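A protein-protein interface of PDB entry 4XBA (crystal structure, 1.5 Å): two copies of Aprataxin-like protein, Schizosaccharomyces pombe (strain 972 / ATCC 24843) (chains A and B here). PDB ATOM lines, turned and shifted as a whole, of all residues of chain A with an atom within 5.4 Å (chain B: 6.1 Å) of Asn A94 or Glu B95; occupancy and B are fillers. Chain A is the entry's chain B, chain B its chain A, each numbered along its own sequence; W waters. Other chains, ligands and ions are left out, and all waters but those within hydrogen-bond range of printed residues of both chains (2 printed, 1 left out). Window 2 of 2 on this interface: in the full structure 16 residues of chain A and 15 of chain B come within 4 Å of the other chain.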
ATOM      1  N   SER A  77     -15.111 -24.448  -5.347  1.00  0.00           N
ATOM      2  CA  SER A  77     -15.367 -24.755  -6.744  1.00  0.00           C
ATOM      3  C   SER A  77     -15.528 -23.475  -7.566  1.00  0.00           C
ATOM      4  O   SER A  77     -14.996 -23.405  -8.662  1.00  0.00           O
ATOM      5  CB  SER A  77     -16.607 -25.657  -6.912  1.00  0.00           C
ATOM      6  OG  SER A  77     -17.791 -24.910  -6.715  1.00  0.00           O
ATOM      7  N   PHE A  81     -13.209 -22.545 -10.872  1.00  0.00           N
ATOM      8  CA  PHE A  81     -13.701 -22.259 -12.199  1.00  0.00           C
ATOM      9  C   PHE A  81     -13.326 -20.859 -12.652  1.00  0.00           C
ATOM     10  O   PHE A  81     -13.043 -20.659 -13.826  1.00  0.00           O
ATOM     11  CB  PHE A  81     -15.241 -22.418 -12.247  1.00  0.00           C
ATOM     12  CG  PHE A  81     -15.711 -23.833 -12.142  1.00  0.00           C
ATOM     13  CD1 PHE A  81     -15.261 -24.796 -13.016  1.00  0.00           C
ATOM     14  CD2 PHE A  81     -16.641 -24.191 -11.177  1.00  0.00           C
ATOM     15  CE1 PHE A  81     -15.700 -26.114 -12.901  1.00  0.00           C
ATOM     16  CE2 PHE A  81     -17.089 -25.505 -11.082  1.00  0.00           C
ATOM     17  CZ  PHE A  81     -16.629 -26.448 -11.935  1.00  0.00           C
ATOM     18  N   ARG A  85     -11.180 -19.781 -15.939  1.00  0.00           N
ATOM     19  CA  ARG A  85     -11.591 -18.763 -16.899  1.00  0.00           C
ATOM     20  C   ARG A  85     -10.490 -17.718 -17.099  1.00  0.00           C
ATOM     21  O   ARG A  85     -10.277 -17.277 -18.204  1.00  0.00           O
ATOM     22  CB  ARG A  85     -12.890 -18.092 -16.469  1.00  0.00           C
ATOM     23  CG  ARG A  85     -14.168 -18.822 -16.957  1.00  0.00           C
ATOM     24  CD  ARG A  85     -15.435 -18.027 -16.531  1.00  0.00           C
ATOM     25  NE  ARG A  85     -15.746 -18.219 -15.113  1.00  0.00           N
ATOM     26  CZ  ARG A  85     -16.415 -19.277 -14.636  1.00  0.00           C
ATOM     27  NH1 ARG A  85     -16.830 -20.217 -15.463  1.00  0.00           N
ATOM     28  NH2 ARG A  85     -16.630 -19.404 -13.338  1.00  0.00           N
ATOM     29  N   LEU A  92     -15.870 -19.424 -21.001  1.00  0.00           N
ATOM     30  CA  LEU A  92     -16.145 -20.802 -20.602  1.00  0.00           C
ATOM     31  C   LEU A  92     -17.019 -20.888 -19.369  1.00  0.00           C
ATOM     32  O   LEU A  92     -16.705 -20.330 -18.330  1.00  0.00           O
ATOM     33  CB  LEU A  92     -14.827 -21.541 -20.351  1.00  0.00           C
ATOM     34  CG  LEU A  92     -13.957 -21.778 -21.591  1.00  0.00           C
ATOM     35  CD1 LEU A  92     -12.531 -22.155 -21.187  1.00  0.00           C
ATOM     36  CD2 LEU A  92     -14.547 -22.856 -22.506  1.00  0.00           C
ATOM     37  N   THR A  93     -18.101 -21.646 -19.490  1.00  0.00           N
ATOM     38  CA  THR A  93     -18.975 -21.931 -18.368  1.00  0.00           C
ATOM     39  C   THR A  93     -18.391 -22.980 -17.432  1.00  0.00           C
ATOM     40  O   THR A  93     -17.476 -23.731 -17.801  1.00  0.00           O
ATOM     41  CB  THR A  93     -20.312 -22.459 -18.853  1.00  0.00           C
ATOM     42  OG1 THR A  93     -20.111 -23.718 -19.510  1.00  0.00           O
ATOM     43  CG2 THR A  93     -20.976 -21.463 -19.794  1.00  0.00           C
ATOM     44  N   ASN A  94     -18.938 -23.048 -16.222  1.00  0.00           N
ATOM     45  CA  ASN A  94     -18.518 -24.069 -15.264  1.00  0.00           C
ATOM     46  C   ASN A  94     -18.758 -25.471 -15.812  1.00  0.00           C
ATOM     47  O   ASN A  94     -17.946 -26.381 -15.611  1.00  0.00           O
ATOM     48  CB  ASN A  94     -19.273 -23.924 -13.941  1.00  0.00           C
ATOM     49  CG  ASN A  94     -18.952 -22.656 -13.195  1.00  0.00           C
ATOM     50  OD1 ASN A  94     -18.078 -21.875 -13.581  1.00  0.00           O
ATOM     51  ND2 ASN A  94     -19.683 -22.432 -12.075  1.00  0.00           N
ATOM     52  N   GLU A  95     -19.861 -25.632 -16.538  1.00  0.00           N
ATOM     53  CA  GLU A  95     -20.201 -26.921 -17.103  1.00  0.00           C
ATOM     54  C   GLU A  95     -19.194 -27.370 -18.170  1.00  0.00           C
ATOM     55  O   GLU A  95     -18.844 -28.546 -18.240  1.00  0.00           O
ATOM     56  CB  GLU A  95     -21.625 -26.860 -17.673  1.00  0.00           C
ATOM     57  CG  GLU A  95     -22.725 -26.706 -16.602  1.00  0.00           C
ATOM     58  CD  GLU A  95     -23.005 -25.248 -16.164  1.00  0.00           C
ATOM     59  OE1 GLU A  95     -23.927 -25.070 -15.320  1.00  0.00           O
ATOM     60  OE2 GLU A  95     -22.324 -24.289 -16.640  1.00  0.00           O
ATOM     61  N   ALA A  96     -18.723 -26.439 -18.983  1.00  0.00           N
ATOM     62  CA  ALA A  96     -17.705 -26.787 -19.980  1.00  0.00           C
ATOM     63  C   ALA A  96     -16.405 -27.181 -19.294  1.00  0.00           C
ATOM     64  O   ALA A  96     -15.691 -28.091 -19.726  1.00  0.00           O
ATOM     65  CB  ALA A  96     -17.465 -25.620 -20.930  1.00  0.00           C
ATOM     66  N   LEU A  97     -16.102 -26.489 -18.210  1.00  0.00           N
ATOM     67  CA  LEU A  97     -14.839 -26.706 -17.512  1.00  0.00           C
ATOM     68  C   LEU A  97     -14.807 -27.925 -16.628  1.00  0.00           C
ATOM     69  O   LEU A  97     -13.746 -28.499 -16.399  1.00  0.00           O
ATOM     70  CB  LEU A  97     -14.484 -25.493 -16.669  1.00  0.00           C
ATOM     71  CG  LEU A  97     -14.005 -24.263 -17.442  1.00  0.00           C
ATOM     72  CD1 LEU A  97     -14.106 -23.003 -16.534  1.00  0.00           C
ATOM     73  CD2 LEU A  97     -12.588 -24.523 -17.907  1.00  0.00           C
ATOM     74  N   CYS A  98     -15.950 -28.351 -16.136  1.00  0.00           N
ATOM     75  CA  CYS A  98     -15.931 -29.421 -15.167  1.00  0.00           C
ATOM     76  C   CYS A  98     -15.402 -30.717 -15.782  1.00  0.00           C
ATOM     77  O   CYS A  98     -14.733 -31.498 -15.114  1.00  0.00           O
ATOM     78  CB  CYS A  98     -17.313 -29.607 -14.607  1.00  0.00           C
ATOM     79  SG  CYS A  98     -18.501 -29.991 -15.859  1.00  0.00           S
ATOM     80  N   ASN A  99     -15.646 -30.902 -17.072  1.00  0.00           N
ATOM     81  CA  ASN A  99     -15.163 -32.075 -17.758  1.00  0.00           C
ATOM     82  C   ASN A  99     -13.718 -31.897 -18.194  1.00  0.00           C
ATOM     83  O   ASN A  99     -13.130 -32.816 -18.749  1.00  0.00           O
ATOM     84  CB  ASN A  99     -16.038 -32.360 -18.976  1.00  0.00           C
ATOM     85  CG  ASN A  99     -17.378 -32.946 -18.598  1.00  0.00           C
ATOM     86  OD1 ASN A  99     -17.468 -33.871 -17.778  1.00  0.00           O
ATOM     87  ND2 ASN A  99     -18.438 -32.395 -19.182  1.00  0.00           N
ATOM     88  N   PHE B  81     -29.571 -31.923 -16.978  1.00  0.00           N
ATOM     89  CA  PHE B  81     -29.401 -31.621 -15.546  1.00  0.00           C
ATOM     90  C   PHE B  81     -30.727 -31.522 -14.820  1.00  0.00           C
ATOM     91  O   PHE B  81     -30.820 -31.940 -13.679  1.00  0.00           O
ATOM     92  CB  PHE B  81     -28.597 -30.316 -15.362  1.00  0.00           C
ATOM     93  CG  PHE B  81     -27.118 -30.445 -15.727  1.00  0.00           C
ATOM     94  CD1 PHE B  81     -26.308 -31.362 -15.113  1.00  0.00           C
ATOM     95  CD2 PHE B  81     -26.572 -29.585 -16.654  1.00  0.00           C
ATOM     96  CE1 PHE B  81     -24.958 -31.459 -15.443  1.00  0.00           C
ATOM     97  CE2 PHE B  81     -25.234 -29.655 -16.972  1.00  0.00           C
ATOM     98  CZ  PHE B  81     -24.446 -30.579 -16.363  1.00  0.00           C
ATOM     99  N   LEU B  92     -29.368 -30.607  -5.990  1.00  0.00           N
ATOM    100  CA  LEU B  92     -28.076 -30.849  -6.646  1.00  0.00           C
ATOM    101  C   LEU B  92     -27.837 -29.817  -7.722  1.00  0.00           C
ATOM    102  O   LEU B  92     -28.660 -29.644  -8.624  1.00  0.00           O
ATOM    103  CB  LEU B  92     -28.026 -32.235  -7.279  1.00  0.00           C
ATOM    104  CG  LEU B  92     -28.052 -33.390  -6.284  1.00  0.00           C
ATOM    105  CD1 LEU B  92     -28.463 -34.733  -6.917  1.00  0.00           C
ATOM    106  CD2 LEU B  92     -26.745 -33.502  -5.534  1.00  0.00           C
ATOM    107  N   THR B  93     -26.718 -29.125  -7.633  1.00  0.00           N
ATOM    108  CA  THR B  93     -26.376 -28.191  -8.669  1.00  0.00           C
ATOM    109  C   THR B  93     -25.826 -28.869  -9.914  1.00  0.00           C
ATOM    110  O   THR B  93     -25.444 -30.033  -9.890  1.00  0.00           O
ATOM    111  CB  THR B  93     -25.329 -27.223  -8.195  1.00  0.00           C
ATOM    112  OG1 THR B  93     -24.176 -27.992  -7.856  1.00  0.00           O
ATOM    113  CG2 THR B  93     -25.828 -26.452  -6.977  1.00  0.00           C
ATOM    114  N   ASN B  94     -25.760 -28.105 -11.000  1.00  0.00           N
ATOM    115  CA  ASN B  94     -25.147 -28.630 -12.221  1.00  0.00           C
ATOM    116  C   ASN B  94     -23.726 -29.033 -11.919  1.00  0.00           C
ATOM    117  O   ASN B  94     -23.236 -30.032 -12.450  1.00  0.00           O
ATOM    118  CB  ASN B  94     -25.140 -27.612 -13.376  1.00  0.00           C
ATOM    119  CG  ASN B  94     -26.498 -27.328 -13.919  1.00  0.00           C
ATOM    120  OD1 ASN B  94     -27.490 -27.938 -13.518  1.00  0.00           O
ATOM    121  ND2 ASN B  94     -26.560 -26.452 -14.902  1.00  0.00           N
ATOM    122  N   GLU B  95     -23.079 -28.272 -11.044  1.00  0.00           N
ATOM    123  CA  GLU B  95     -21.694 -28.565 -10.694  1.00  0.00           C
ATOM    124  C   GLU B  95     -21.561 -29.896  -9.961  1.00  0.00           C
ATOM    125  O   GLU B  95     -20.643 -30.666 -10.205  1.00  0.00           O
ATOM    126  CB  GLU B  95     -21.114 -27.404  -9.872  1.00  0.00           C
ATOM    127  CG  GLU B  95     -20.893 -26.120 -10.731  1.00  0.00           C
ATOM    128  CD  GLU B  95     -22.121 -25.207 -10.898  1.00  0.00           C
ATOM    129  OE1 GLU B  95     -22.003 -24.143 -11.551  1.00  0.00           O
ATOM    130  OE2 GLU B  95     -23.215 -25.528 -10.400  1.00  0.00           O
ATOM    131  N   ALA B  96     -22.491 -30.184  -9.071  1.00  0.00           N
ATOM    132  CA  ALA B  96     -22.468 -31.490  -8.395  1.00  0.00           C
ATOM    133  C   ALA B  96     -22.729 -32.642  -9.372  1.00  0.00           C
ATOM    134  O   ALA B  96     -22.099 -33.722  -9.318  1.00  0.00           O
ATOM    135  CB  ALA B  96     -23.483 -31.506  -7.303  1.00  0.00           C
ATOM    136  N   LEU B  97     -23.641 -32.410 -10.302  1.00  0.00           N
ATOM    137  CA  LEU B  97     -24.062 -33.459 -11.221  1.00  0.00           C
ATOM    138  C   LEU B  97     -23.098 -33.766 -12.356  1.00  0.00           C
ATOM    139  O   LEU B  97     -23.059 -34.850 -12.862  1.00  0.00           O
ATOM    140  CB  LEU B  97     -25.391 -33.084 -11.845  1.00  0.00           C
ATOM    141  CG  LEU B  97     -26.512 -33.197 -10.826  1.00  0.00           C
ATOM    142  CD1 LEU B  97     -27.697 -32.410 -11.362  1.00  0.00           C
ATOM    143  CD2 LEU B  97     -26.868 -34.630 -10.609  1.00  0.00           C
ATOM    144  N   CYS B  98     -22.314 -32.771 -12.747  1.00  0.00           N
ATOM    145  CA  CYS B  98     -21.412 -32.947 -13.882  1.00  0.00           C
ATOM    146  C   CYS B  98     -20.475 -34.115 -13.664  1.00  0.00           C
ATOM    147  O   CYS B  98     -20.187 -34.891 -14.593  1.00  0.00           O
ATOM    148  CB  CYS B  98     -20.599 -31.687 -14.086  1.00  0.00           C
ATOM    149  SG  CYS B  98     -21.231 -30.610 -15.335  1.00  0.00           S
ATOM    150  N   ASN B  99     -20.029 -34.263 -12.429  1.00  0.00           N
ATOM    151  CA  ASN B  99     -19.086 -35.303 -12.106  1.00  0.00           C
ATOM    152  C   ASN B  99     -19.771 -36.659 -11.873  1.00  0.00           C
ATOM    153  O   ASN B  99     -19.102 -37.666 -11.656  1.00  0.00           O
ATOM    154  CB  ASN B  99     -18.242 -34.890 -10.894  1.00  0.00           C
ATOM    155  CG  ASN B  99     -17.129 -33.898 -11.270  1.00  0.00           C
ATOM    156  OD1 ASN B  99     -16.397 -34.100 -12.250  1.00  0.00           O
ATOM    157  ND2 ASN B  99     -17.017 -32.819 -10.508  1.00  0.00           N
HETATM  158  O   HOH W   1     -22.744 -23.217 -13.650  1.00  0.00           O
HETATM  159  O   HOH W   2     -13.452 -32.401 -12.977  1.00  0.00           O
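The side-chain amide nitrogen (ND2) of Asn B94 sits at hydrogen-bond distance from the side-chain carboxylate (OE1) of Glu A95.
The side-chain carboxylate of Glu B95 is in hydrogen-bond range of the side-chain amide nitrogen of Asn A94, 2.9 Å away.
The side-chain sulfur of Cys B98 sits close to the side-chain sulfur of Cys A98.
Among the printed residues, pairs that only touch across the chains: Phe A81 with Glu B95 and Glu A95 with Phe B81.
OG1 of Thr B93 lies close to N of Glu B95 (3.4 Å).
The backbone carbonyl oxygen (O) of Asn B94 lies close to the side-chain sulfur (SG) of Cys B98, 3.6 Å away.
OD1 of Asn A94 is in hydrogen-bond range of NH1 of Arg A85 (2.8 Å).
SG of Cys A98 lies close to O of Asn A94 (3.7 Å).
The backbone carbonyl oxygen (O) of Glu A95 is in hydrogen-bond range of the side-chain sulfur (SG) of Cys A98, 2.8 Å away.
Of the 11 printed residues of chain A, 4 touch a printed residue of chain B.
Hydrophobic or aromatic side chains of chain A that line the printed part of chain B: Phe A81.
Among the printed residues, 5 pairs touch across the chains.
Among the printed residues, no Asp or Glu carboxylate lies within 4 Å of a Lys or Arg side-chain nitrogen of the other chain.
Water W1 lies within hydrogen-bond range of OE1 of Glu B95 (2.4 Å) and OE1 of Glu A95 (2.8 Å).
Water W2 lies within hydrogen-bond range of O of Cys A98 (2.7 Å) and OD1 of Asn B99 (3.5 Å).
Phe A81 touches Glu B95, and with the chains exchanged Glu A95 touches Phe B81.
Asn A94 touches Glu B95, and with the chains exchanged Glu A95 touches Asn B94.
Cys A98 touches its own counterpart, Cys B98.
Of the printed residues of chain A, Asn B94 touches Glu A95 (3.0 Å).
Of the printed residues of chain B, Glu A95 touches Phe B81 (3.9 Å) and Asn B94 (3.0 Å).
Printed residues of chain B within 4 Å of Phe A81: Glu B95 (3.9 Å).
Of the printed residues of chain B, Cys A98 touches Cys B98 (2.8 Å).
The nearest printed residue of chain B that does not touch Asn A94 is Cys B98 (5.4 Å).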
